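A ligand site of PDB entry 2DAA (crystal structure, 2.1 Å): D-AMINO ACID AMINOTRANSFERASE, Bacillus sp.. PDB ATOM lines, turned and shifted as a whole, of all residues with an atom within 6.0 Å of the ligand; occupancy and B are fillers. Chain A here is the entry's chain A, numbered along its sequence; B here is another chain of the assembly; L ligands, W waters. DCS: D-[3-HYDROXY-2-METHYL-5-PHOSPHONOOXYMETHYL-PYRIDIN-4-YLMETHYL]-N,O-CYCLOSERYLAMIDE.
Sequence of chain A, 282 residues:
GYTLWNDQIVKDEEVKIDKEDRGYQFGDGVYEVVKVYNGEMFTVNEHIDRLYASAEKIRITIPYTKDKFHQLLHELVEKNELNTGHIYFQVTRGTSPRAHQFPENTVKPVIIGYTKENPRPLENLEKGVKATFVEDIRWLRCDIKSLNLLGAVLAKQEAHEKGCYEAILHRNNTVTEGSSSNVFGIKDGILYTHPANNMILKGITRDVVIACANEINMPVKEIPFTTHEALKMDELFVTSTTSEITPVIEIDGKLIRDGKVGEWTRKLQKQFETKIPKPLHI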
ATOM      1  N   TYR A  31     -24.262 -36.699 -28.175  1.00  0.00           N
ATOM      2  CA  TYR A  31     -23.176 -36.963 -29.110  1.00  0.00           C
ATOM      3  C   TYR A  31     -21.771 -36.684 -28.551  1.00  0.00           C
ATOM      4  O   TYR A  31     -21.621 -36.167 -27.441  1.00  0.00           O
ATOM      5  CB  TYR A  31     -23.375 -36.146 -30.385  1.00  0.00           C
ATOM      6  CG  TYR A  31     -23.051 -34.676 -30.226  1.00  0.00           C
ATOM      7  CD1 TYR A  31     -23.954 -33.790 -29.641  1.00  0.00           C
ATOM      8  CD2 TYR A  31     -21.818 -34.157 -30.648  1.00  0.00           C
ATOM      9  CE1 TYR A  31     -23.646 -32.435 -29.464  1.00  0.00           C
ATOM     10  CE2 TYR A  31     -21.505 -32.817 -30.488  1.00  0.00           C
ATOM     11  CZ  TYR A  31     -22.410 -31.967 -29.895  1.00  0.00           C
ATOM     12  OH  TYR A  31     -22.081 -30.643 -29.740  1.00  0.00           O
ATOM     13  N   GLU A  32     -20.760 -37.029 -29.345  1.00  0.00           N
ATOM     14  CA  GLU A  32     -19.363 -36.788 -29.010  1.00  0.00           C
ATOM     15  C   GLU A  32     -18.554 -36.566 -30.276  1.00  0.00           C
ATOM     16  O   GLU A  32     -18.989 -36.888 -31.387  1.00  0.00           O
ATOM     17  CB  GLU A  32     -18.755 -37.981 -28.280  1.00  0.00           C
ATOM     18  CG  GLU A  32     -19.084 -38.075 -26.815  1.00  0.00           C
ATOM     19  CD  GLU A  32     -18.586 -36.900 -26.005  1.00  0.00           C
ATOM     20  OE1 GLU A  32     -17.748 -36.112 -26.483  1.00  0.00           O
ATOM     21  OE2 GLU A  32     -19.060 -36.770 -24.867  1.00  0.00           O
ATOM     22  N   VAL A  33     -17.359 -36.000 -30.093  1.00  0.00           N
ATOM     23  CA  VAL A  33     -16.403 -35.726 -31.161  1.00  0.00           C
ATOM     24  C   VAL A  33     -15.030 -36.076 -30.574  1.00  0.00           C
ATOM     25  O   VAL A  33     -14.680 -35.589 -29.491  1.00  0.00           O
ATOM     26  CB  VAL A  33     -16.414 -34.233 -31.594  1.00  0.00           C
ATOM     27  CG1 VAL A  33     -15.302 -33.955 -32.599  1.00  0.00           C
ATOM     28  CG2 VAL A  33     -17.734 -33.882 -32.208  1.00  0.00           C
ATOM     29  N   HIS A  47     -13.990 -39.375 -23.598  1.00  0.00           N
ATOM     30  CA  HIS A  47     -15.139 -39.035 -24.429  1.00  0.00           C
ATOM     31  C   HIS A  47     -16.245 -40.090 -24.362  1.00  0.00           C
ATOM     32  O   HIS A  47     -17.418 -39.761 -24.419  1.00  0.00           O
ATOM     33  CB  HIS A  47     -14.719 -38.803 -25.881  1.00  0.00           C
ATOM     34  CG  HIS A  47     -14.079 -37.477 -26.112  1.00  0.00           C
ATOM     35  ND1 HIS A  47     -14.794 -36.344 -26.426  1.00  0.00           N
ATOM     36  CD2 HIS A  47     -12.769 -37.092 -26.099  1.00  0.00           C
ATOM     37  CE1 HIS A  47     -13.971 -35.328 -26.599  1.00  0.00           C
ATOM     38  NE2 HIS A  47     -12.741 -35.754 -26.396  1.00  0.00           N
ATOM     39  N   ARG A  50     -18.175 -39.818 -21.056  1.00  0.00           N
ATOM     40  CA  ARG A  50     -19.086 -38.683 -21.141  1.00  0.00           C
ATOM     41  C   ARG A  50     -20.319 -38.968 -21.983  1.00  0.00           C
ATOM     42  O   ARG A  50     -21.408 -38.492 -21.671  1.00  0.00           O
ATOM     43  CB  ARG A  50     -18.364 -37.419 -21.629  1.00  0.00           C
ATOM     44  CG  ARG A  50     -19.128 -36.156 -21.281  1.00  0.00           C
ATOM     45  CD  ARG A  50     -18.318 -34.914 -21.613  1.00  0.00           C
ATOM     46  NE  ARG A  50     -18.125 -34.769 -23.047  1.00  0.00           N
ATOM     47  CZ  ARG A  50     -17.513 -33.749 -23.620  1.00  0.00           C
ATOM     48  NH1 ARG A  50     -17.006 -32.765 -22.890  1.00  0.00           N
ATOM     49  NH2 ARG A  50     -17.406 -33.694 -24.934  1.00  0.00           N
ATOM     50  N   TYR A  88     -17.090 -38.388 -35.380  1.00  0.00           N
ATOM     51  CA  TYR A  88     -18.317 -37.831 -34.834  1.00  0.00           C
ATOM     52  C   TYR A  88     -19.217 -39.024 -34.615  1.00  0.00           C
ATOM     53  O   TYR A  88     -19.288 -39.896 -35.469  1.00  0.00           O
ATOM     54  CB  TYR A  88     -18.983 -36.855 -35.823  1.00  0.00           C
ATOM     55  CG  TYR A  88     -20.376 -36.436 -35.384  1.00  0.00           C
ATOM     56  CD1 TYR A  88     -20.557 -35.353 -34.509  1.00  0.00           C
ATOM     57  CD2 TYR A  88     -21.502 -37.150 -35.776  1.00  0.00           C
ATOM     58  CE1 TYR A  88     -21.821 -35.020 -34.034  1.00  0.00           C
ATOM     59  CE2 TYR A  88     -22.773 -36.824 -35.304  1.00  0.00           C
ATOM     60  CZ  TYR A  88     -22.926 -35.755 -34.438  1.00  0.00           C
ATOM     61  OH  TYR A  88     -24.181 -35.434 -33.962  1.00  0.00           O
ATOM     62  N   ARG A 138     -29.854 -20.464 -24.147  1.00  0.00           N
ATOM     63  CA  ARG A 138     -30.033 -21.901 -24.211  1.00  0.00           C
ATOM     64  C   ARG A 138     -30.788 -22.439 -23.002  1.00  0.00           C
ATOM     65  O   ARG A 138     -31.028 -21.727 -22.036  1.00  0.00           O
ATOM     66  CB  ARG A 138     -28.681 -22.593 -24.336  1.00  0.00           C
ATOM     67  CG  ARG A 138     -27.901 -22.180 -25.591  1.00  0.00           C
ATOM     68  CD  ARG A 138     -26.499 -22.784 -25.598  1.00  0.00           C
ATOM     69  NE  ARG A 138     -25.726 -22.318 -24.463  1.00  0.00           N
ATOM     70  CZ  ARG A 138     -24.693 -22.957 -23.944  1.00  0.00           C
ATOM     71  NH1 ARG A 138     -24.269 -24.103 -24.472  1.00  0.00           N
ATOM     72  NH2 ARG A 138     -24.098 -22.474 -22.860  1.00  0.00           N
ATOM     73  N   LYS A 145     -24.660 -33.125 -23.208  1.00  0.00           N
ATOM     74  CA  LYS A 145     -24.219 -32.855 -24.570  1.00  0.00           C
ATOM     75  C   LYS A 145     -25.245 -33.453 -25.537  1.00  0.00           C
ATOM     76  O   LYS A 145     -25.010 -34.497 -26.142  1.00  0.00           O
ATOM     77  CB  LYS A 145     -22.821 -33.441 -24.788  1.00  0.00           C
ATOM     78  CG  LYS A 145     -22.081 -32.941 -26.017  1.00  0.00           C
ATOM     79  CD  LYS A 145     -20.657 -33.494 -26.037  1.00  0.00           C
ATOM     80  CE  LYS A 145     -19.836 -33.057 -27.250  1.00  0.00           C
ATOM     81  NZ  LYS A 145     -19.374 -31.650 -27.193  1.00  0.00           N
ATOM     82  N   LEU A 149     -29.235 -28.233 -30.304  1.00  0.00           N
ATOM     83  CA  LEU A 149     -28.198 -27.219 -30.495  1.00  0.00           C
ATOM     84  C   LEU A 149     -28.571 -25.951 -31.242  1.00  0.00           C
ATOM     85  O   LEU A 149     -27.676 -25.205 -31.662  1.00  0.00           O
ATOM     86  CB  LEU A 149     -26.988 -27.843 -31.204  1.00  0.00           C
ATOM     87  CG  LEU A 149     -26.292 -28.999 -30.490  1.00  0.00           C
ATOM     88  CD1 LEU A 149     -25.486 -29.824 -31.493  1.00  0.00           C
ATOM     89  CD2 LEU A 149     -25.415 -28.457 -29.381  1.00  0.00           C
ATOM     90  N   GLU A 177     -19.848 -20.080 -21.422  1.00  0.00           N
ATOM     91  CA  GLU A 177     -18.965 -20.825 -22.322  1.00  0.00           C
ATOM     92  C   GLU A 177     -19.164 -20.290 -23.735  1.00  0.00           C
ATOM     93  O   GLU A 177     -19.878 -19.307 -23.925  1.00  0.00           O
ATOM     94  CB  GLU A 177     -19.275 -22.342 -22.271  1.00  0.00           C
ATOM     95  CG  GLU A 177     -20.692 -22.719 -22.708  1.00  0.00           C
ATOM     96  CD  GLU A 177     -20.980 -24.198 -22.597  1.00  0.00           C
ATOM     97  OE1 GLU A 177     -20.027 -24.992 -22.470  1.00  0.00           O
ATOM     98  OE2 GLU A 177     -22.160 -24.586 -22.649  1.00  0.00           O
ATOM     99  N   GLY A 178     -18.470 -20.873 -24.723  1.00  0.00           N
ATOM    100  CA  GLY A 178     -18.632 -20.413 -26.092  1.00  0.00           C
ATOM    101  C   GLY A 178     -19.668 -21.266 -26.807  1.00  0.00           C
ATOM    102  O   GLY A 178     -20.042 -22.315 -26.285  1.00  0.00           O
ATOM    103  N   SER A 179     -20.117 -20.855 -27.988  1.00  0.00           N
ATOM    104  CA  SER A 179     -21.110 -21.651 -28.715  1.00  0.00           C
ATOM    105  C   SER A 179     -20.672 -23.109 -28.925  1.00  0.00           C
ATOM    106  O   SER A 179     -21.520 -23.997 -29.063  1.00  0.00           O
ATOM    107  CB  SER A 179     -21.504 -20.980 -30.025  1.00  0.00           C
ATOM    108  OG  SER A 179     -20.389 -20.812 -30.867  1.00  0.00           O
ATOM    109  N   SER A 180     -19.359 -23.353 -29.008  1.00  0.00           N
ATOM    110  CA  SER A 180     -18.858 -24.731 -29.113  1.00  0.00           C
ATOM    111  C   SER A 180     -17.479 -24.889 -28.480  1.00  0.00           C
ATOM    112  O   SER A 180     -16.631 -25.634 -28.981  1.00  0.00           O
ATOM    113  CB  SER A 180     -18.852 -25.252 -30.558  1.00  0.00           C
ATOM    114  OG  SER A 180     -17.860 -24.644 -31.343  1.00  0.00           O
ATOM    115  N   SER A 181     -17.265 -24.226 -27.342  1.00  0.00           N
ATOM    116  CA  SER A 181     -15.987 -24.304 -26.630  1.00  0.00           C
ATOM    117  C   SER A 181     -16.167 -23.807 -25.205  1.00  0.00           C
ATOM    118  O   SER A 181     -17.237 -23.296 -24.848  1.00  0.00           O
ATOM    119  CB  SER A 181     -14.952 -23.420 -27.325  1.00  0.00           C
ATOM    120  OG  SER A 181     -15.333 -22.054 -27.280  1.00  0.00           O
ATOM    121  N   ASN A 182     -15.160 -24.057 -24.361  1.00  0.00           N
ATOM    122  CA  ASN A 182     -15.180 -23.569 -22.973  1.00  0.00           C
ATOM    123  C   ASN A 182     -14.309 -22.311 -22.961  1.00  0.00           C
ATOM    124  O   ASN A 182     -13.432 -22.162 -23.814  1.00  0.00           O
ATOM    125  CB  ASN A 182     -14.668 -24.622 -21.992  1.00  0.00           C
ATOM    126  CG  ASN A 182     -15.708 -25.685 -21.690  1.00  0.00           C
ATOM    127  OD1 ASN A 182     -15.516 -26.864 -22.001  1.00  0.00           O
ATOM    128  ND2 ASN A 182     -16.824 -25.279 -21.081  1.00  0.00           N
ATOM    129  N   LEU A 201     -20.917 -27.123 -20.297  1.00  0.00           N
ATOM    130  CA  LEU A 201     -20.544 -28.505 -20.629  1.00  0.00           C
ATOM    131  C   LEU A 201     -19.160 -28.678 -20.012  1.00  0.00           C
ATOM    132  O   LEU A 201     -18.309 -27.807 -20.180  1.00  0.00           O
ATOM    133  CB  LEU A 201     -20.433 -28.672 -22.152  1.00  0.00           C
ATOM    134  CG  LEU A 201     -20.759 -30.004 -22.848  1.00  0.00           C
ATOM    135  CD1 LEU A 201     -19.735 -30.227 -23.941  1.00  0.00           C
ATOM    136  CD2 LEU A 201     -20.725 -31.174 -21.896  1.00  0.00           C
ATOM    137  N   LYS A 202     -18.947 -29.746 -19.252  1.00  0.00           N
ATOM    138  CA  LYS A 202     -17.642 -30.004 -18.641  1.00  0.00           C
ATOM    139  C   LYS A 202     -16.784 -30.596 -19.756  1.00  0.00           C
ATOM    140  O   LYS A 202     -16.727 -31.814 -19.924  1.00  0.00           O
ATOM    141  CB  LYS A 202     -17.804 -30.997 -17.487  1.00  0.00           C
ATOM    142  CG  LYS A 202     -16.610 -31.129 -16.548  1.00  0.00           C
ATOM    143  CD  LYS A 202     -16.944 -32.093 -15.419  1.00  0.00           C
ATOM    144  CE  LYS A 202     -15.856 -32.164 -14.360  1.00  0.00           C
ATOM    145  NZ  LYS A 202     -14.665 -32.950 -14.780  1.00  0.00           N
ATOM    146  N   GLY A 203     -16.138 -29.732 -20.538  1.00  0.00           N
ATOM    147  CA  GLY A 203     -15.316 -30.167 -21.659  1.00  0.00           C
ATOM    148  C   GLY A 203     -14.130 -31.058 -21.332  1.00  0.00           C
ATOM    149  O   GLY A 203     -13.548 -30.938 -20.261  1.00  0.00           O
ATOM    150  N   ILE A 204     -13.763 -31.921 -22.267  1.00  0.00           N
ATOM    151  CA  ILE A 204     -12.639 -32.820 -22.047  1.00  0.00           C
ATOM    152  C   ILE A 204     -11.349 -32.003 -22.171  1.00  0.00           C
ATOM    153  O   ILE A 204     -10.456 -32.145 -21.347  1.00  0.00           O
ATOM    154  CB  ILE A 204     -12.609 -34.007 -23.056  1.00  0.00           C
ATOM    155  CG1 ILE A 204     -13.889 -34.837 -22.960  1.00  0.00           C
ATOM    156  CG2 ILE A 204     -11.386 -34.901 -22.800  1.00  0.00           C
ATOM    157  CD1 ILE A 204     -14.237 -35.354 -21.567  1.00  0.00           C
ATOM    158  N   THR A 205     -11.306 -31.121 -23.160  1.00  0.00           N
ATOM    159  CA  THR A 205     -10.127 -30.284 -23.364  1.00  0.00           C
ATOM    160  C   THR A 205      -9.943 -29.410 -22.136  1.00  0.00           C
ATOM    161  O   THR A 205      -8.832 -29.196 -21.677  1.00  0.00           O
ATOM    162  CB  THR A 205     -10.276 -29.410 -24.581  1.00  0.00           C
ATOM    163  OG1 THR A 205     -10.793 -30.194 -25.657  1.00  0.00           O
ATOM    164  CG2 THR A 205      -8.925 -28.848 -25.007  1.00  0.00           C
ATOM    165  N   ARG A 206     -11.074 -28.942 -21.619  1.00  0.00           N
ATOM    166  CA  ARG A 206     -11.131 -28.107 -20.421  1.00  0.00           C
ATOM    167  C   ARG A 206     -10.416 -28.797 -19.262  1.00  0.00           C
ATOM    168  O   ARG A 206      -9.526 -28.217 -18.650  1.00  0.00           O
ATOM    169  CB  ARG A 206     -12.600 -27.862 -20.050  1.00  0.00           C
ATOM    170  CG  ARG A 206     -12.838 -27.159 -18.719  1.00  0.00           C
ATOM    171  CD  ARG A 206     -14.327 -27.219 -18.329  1.00  0.00           C
ATOM    172  NE  ARG A 206     -14.616 -26.372 -17.172  1.00  0.00           N
ATOM    173  CZ  ARG A 206     -14.543 -26.772 -15.907  1.00  0.00           C
ATOM    174  NH1 ARG A 206     -14.225 -28.030 -15.610  1.00  0.00           N
ATOM    175  NH2 ARG A 206     -14.810 -25.920 -14.939  1.00  0.00           N
ATOM    176  N   THR A 239     -11.366 -23.456 -25.457  1.00  0.00           N
ATOM    177  CA  THR A 239     -10.945 -24.837 -25.643  1.00  0.00           C
ATOM    178  C   THR A 239     -12.034 -25.754 -26.206  1.00  0.00           C
ATOM    179  O   THR A 239     -13.228 -25.560 -25.931  1.00  0.00           O
ATOM    180  CB  THR A 239     -10.459 -25.448 -24.312  1.00  0.00           C
ATOM    181  OG1 THR A 239     -11.533 -25.438 -23.361  1.00  0.00           O
ATOM    182  CG2 THR A 239      -9.299 -24.672 -23.752  1.00  0.00           C
ATOM    183  N   SER A 240     -11.635 -26.718 -27.020  1.00  0.00           N
ATOM    184  CA  SER A 240     -12.540 -27.711 -27.594  1.00  0.00           C
ATOM    185  C   SER A 240     -11.703 -28.784 -28.276  1.00  0.00           C
ATOM    186  O   SER A 240     -10.524 -28.579 -28.595  1.00  0.00           O
ATOM    187  CB  SER A 240     -13.545 -27.098 -28.566  1.00  0.00           C
ATOM    188  OG  SER A 240     -13.018 -26.945 -29.867  1.00  0.00           O
ATOM    189  N   THR A 241     -12.301 -29.956 -28.451  1.00  0.00           N
ATOM    190  CA  THR A 241     -11.624 -31.081 -29.084  1.00  0.00           C
ATOM    191  C   THR A 241     -11.003 -30.713 -30.441  1.00  0.00           C
ATOM    192  O   THR A 241      -9.913 -31.206 -30.757  1.00  0.00           O
ATOM    193  CB  THR A 241     -12.595 -32.271 -29.217  1.00  0.00           C
ATOM    194  OG1 THR A 241     -12.972 -32.700 -27.901  1.00  0.00           O
ATOM    195  CG2 THR A 241     -11.945 -33.430 -29.935  1.00  0.00           C
ATOM    196  N   THR A 242     -11.627 -29.815 -31.202  1.00  0.00           N
ATOM    197  CA  THR A 242     -11.092 -29.427 -32.501  1.00  0.00           C
ATOM    198  C   THR A 242     -10.284 -28.114 -32.531  1.00  0.00           C
ATOM    199  O   THR A 242      -9.381 -27.960 -33.359  1.00  0.00           O
ATOM    200  CB  THR A 242     -12.188 -29.399 -33.586  1.00  0.00           C
ATOM    201  OG1 THR A 242     -13.237 -28.510 -33.203  1.00  0.00           O
ATOM    202  CG2 THR A 242     -12.776 -30.792 -33.768  1.00  0.00           C
ATOM    203  N   PHE B  26     -28.609 -30.976 -35.352  1.00  0.00           N
ATOM    204  CA  PHE B  26     -28.761 -29.793 -34.501  1.00  0.00           C
ATOM    205  C   PHE B  26     -30.202 -29.465 -34.097  1.00  0.00           C
ATOM    206  O   PHE B  26     -30.426 -28.524 -33.325  1.00  0.00           O
ATOM    207  CB  PHE B  26     -28.196 -28.545 -35.222  1.00  0.00           C
ATOM    208  CG  PHE B  26     -26.745 -28.656 -35.628  1.00  0.00           C
ATOM    209  CD1 PHE B  26     -25.732 -28.370 -34.725  1.00  0.00           C
ATOM    210  CD2 PHE B  26     -26.402 -29.024 -36.926  1.00  0.00           C
ATOM    211  CE1 PHE B  26     -24.394 -28.456 -35.105  1.00  0.00           C
ATOM    212  CE2 PHE B  26     -25.066 -29.113 -37.322  1.00  0.00           C
ATOM    213  CZ  PHE B  26     -24.058 -28.830 -36.406  1.00  0.00           C
ATOM    214  N   ARG B  98     -21.167 -31.244 -41.613  1.00  0.00           N
ATOM    215  CA  ARG B  98     -21.334 -30.717 -40.262  1.00  0.00           C
ATOM    216  C   ARG B  98     -20.524 -29.496 -39.852  1.00  0.00           C
ATOM    217  O   ARG B  98     -19.293 -29.491 -39.909  1.00  0.00           O
ATOM    218  CB  ARG B  98     -21.152 -31.807 -39.212  1.00  0.00           C
ATOM    219  CG  ARG B  98     -21.629 -31.391 -37.830  1.00  0.00           C
ATOM    220  CD  ARG B  98     -21.358 -32.451 -36.789  1.00  0.00           C
ATOM    221  NE  ARG B  98     -21.964 -32.083 -35.507  1.00  0.00           N
ATOM    222  CZ  ARG B  98     -21.334 -31.425 -34.545  1.00  0.00           C
ATOM    223  NH1 ARG B  98     -20.070 -31.076 -34.685  1.00  0.00           N
ATOM    224  NH2 ARG B  98     -21.978 -31.132 -33.428  1.00  0.00           N
ATOM    225  N   HIS B 100     -21.529 -25.787 -37.148  1.00  0.00           N
ATOM    226  CA  HIS B 100     -22.545 -25.037 -36.423  1.00  0.00           C
ATOM    227  C   HIS B 100     -23.157 -23.896 -37.232  1.00  0.00           C
ATOM    228  O   HIS B 100     -24.372 -23.718 -37.242  1.00  0.00           O
ATOM    229  CB  HIS B 100     -21.998 -24.487 -35.100  1.00  0.00           C
ATOM    230  CG  HIS B 100     -21.799 -25.529 -34.051  1.00  0.00           C
ATOM    231  ND1 HIS B 100     -22.558 -25.582 -32.902  1.00  0.00           N
ATOM    232  CD2 HIS B 100     -20.912 -26.549 -33.959  1.00  0.00           C
ATOM    233  CE1 HIS B 100     -22.149 -26.586 -32.145  1.00  0.00           C
ATOM    234  NE2 HIS B 100     -21.148 -27.190 -32.764  1.00  0.00           N
HETATM  235  N1  DCS L   1     -18.989 -26.383 -24.650  1.00  0.00           N
HETATM  236  C2  DCS L   1     -19.735 -26.590 -25.749  1.00  0.00           C
HETATM  237  C2A DCS L   1     -21.075 -25.892 -25.793  1.00  0.00           C
HETATM  238  C3  DCS L   1     -19.332 -27.426 -26.796  1.00  0.00           C
HETATM  239  O3  DCS L   1     -20.215 -27.659 -27.825  1.00  0.00           O
HETATM  240  C4  DCS L   1     -18.044 -28.022 -26.750  1.00  0.00           C
HETATM  241  C4A DCS L   1     -17.516 -28.962 -27.834  1.00  0.00           C
HETATM  242  C5  DCS L   1     -17.243 -27.739 -25.633  1.00  0.00           C
HETATM  243  C6  DCS L   1     -17.774 -26.955 -24.602  1.00  0.00           C
HETATM  244  C5A DCS L   1     -15.861 -28.288 -25.522  1.00  0.00           C
HETATM  245  O4P DCS L   1     -15.967 -29.664 -25.198  1.00  0.00           O
HETATM  246  P   DCS L   1     -14.759 -30.589 -25.518  1.00  0.00           P
HETATM  247  O1P DCS L   1     -14.993 -31.888 -24.866  1.00  0.00           O
HETATM  248  O2P DCS L   1     -14.677 -30.748 -26.996  1.00  0.00           O
HETATM  249  O3P DCS L   1     -13.512 -29.962 -24.986  1.00  0.00           O
HETATM  250  N   DCS L   1     -18.426 -29.174 -28.922  1.00  0.00           N
HETATM  251  CA  DCS L   1     -18.095 -29.678 -30.121  1.00  0.00           C
HETATM  252  C   DCS L   1     -19.016 -29.876 -31.264  1.00  0.00           C
HETATM  253  O   DCS L   1     -20.214 -29.629 -31.224  1.00  0.00           O
HETATM  254  ND  DCS L   1     -18.301 -30.314 -32.301  1.00  0.00           N
HETATM  255  OG  DCS L   1     -16.913 -30.268 -32.029  1.00  0.00           O
HETATM  256  CB  DCS L   1     -16.737 -30.153 -30.621  1.00  0.00           C
HETATM  257  O   HOH W   1     -22.477 -26.455 -29.145  1.00  0.00           O
HETATM  258  O   HOH W   2     -21.907 -29.466 -27.270  1.00  0.00           O
HETATM  259  O   HOH W   3     -16.163 -32.631 -28.186  1.00  0.00           O
HETATM  260  O   HOH W   4     -12.961 -27.787 -23.319  1.00  0.00           O
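OH of Tyr 31 sits at hydrogen-bond distance from O of the ligand (2.6 Å).
An oxygen (O2P) of the ligand lies within hydrogen-bond range of the backbone NH (N) of Thr 241, 2.9 Å away.
OG1 of Thr 241 lies within hydrogen-bond range of O2P of the ligand, at 2.7 Å.
A nitrogen (N1) of the ligand lies within hydrogen-bond range of the side-chain carboxylate (OE1) of Glu 177, at 2.8 Å.
The backbone NH (N) of Thr 205 sits at hydrogen-bond distance from an oxygen (O3P) of the ligand.
An oxygen (O3P) of the ligand sits at hydrogen-bond distance from the side-chain hydroxyl of Thr 205 (2.8 Å).
The backbone NH of Ile 204 is in hydrogen-bond range of an oxygen (O1P) of the ligand (2.9 Å).
An oxygen (O1P) of the ligand lies within salt-bridge range of the guanidinium group of Arg 50, 3.0 Å away.
An oxygen (O) of the ligand lies within hydrogen-bond range of a ring nitrogen (NE2) of His 100 of chain B (3.0 Å).
NH2 of Arg 98 of chain B is in hydrogen-bond range of O of the ligand (3.2 Å).
NZ of Lys 145 sits close to N of the ligand, 3.2 Å away.
N of Tyr 31 lies within hydrogen-bond range of O of Lys 145 (3.1 Å).
The side-chain hydroxyl of Thr 205 lies within hydrogen-bond range of the backbone NH of Thr 241, 3.2 Å away.
OE1 of Glu 177 sits at hydrogen-bond distance from N of Leu 201, 3.2 Å away.
NH1 of Arg 138 is in salt-bridge range of OE2 of Glu 177, 2.8 Å away.
The side-chain hydroxyl (OG1) of Thr 205 sits close to the backbone carbonyl oxygen (O) of Ser 240, 3.4 Å away.
NH1 of Arg 50 sits at hydrogen-bond distance from O of Lys 202 (3.1 Å).
The backbone NH (N) of Gly 203 is in hydrogen-bond range of the side-chain amide oxygen (OD1) of Asn 182 (3.3 Å).
O of Leu 201 sits at hydrogen-bond distance from ND2 of Asn 182, at 3.1 Å.
Merely in contact with the ligand: Val 33 (3.6 Å), His 47 (3.99 Å), Arg 138 (3.9 Å), Gly 178 (3.8 Å), Ser 179 (3.8 Å), Ser 180 (3.5 Å), Ser 181 (3.6 Å), Asn 182 (3.4 Å), Leu 201 (3.7 Å), Gly 203 (3.6 Å), Thr 239 (3.8 Å) and Ser 240 (3.6 Å).
21 residues have an atom within 4 Å of the ligand: Tyr 31, Val 33, His 47, Arg 50, Arg 138, Lys 145, Glu 177, Gly 178, Ser 179, Ser 180, Ser 181, Asn 182, Leu 201, Gly 203, Ile 204, Thr 205, Thr 239, Ser 240, Thr 241, Arg 98 of chain B and His 100 of chain B.
Along chain A the residues within 4 Å of the ligand span positions 31 to 241.
The nearest printed residue that does not touch the ligand is Thr 242 (4.2 Å).
Water W2 lies within hydrogen-bond range of an oxygen (O3) of the ligand, the side-chain hydroxyl (OH) of Tyr 31 and the side-chain amino group (NZ) of Lys 145.
Water W3 bridges O2P of the ligand (2.7 Å) and OG1 of Thr 241 (3.2 Å).
Water W4 lies within hydrogen-bond range of the side-chain hydroxyl of Thr 239 (2.7 Å), the backbone NH of Arg 206 (2.8 Å), an oxygen (O3P) of the ligand (2.8 Å) and the side-chain amide oxygen of Asn 182 (3.0 Å).
Water W1 lies within hydrogen-bond range of O of Ser 179 and O3 of the ligand.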
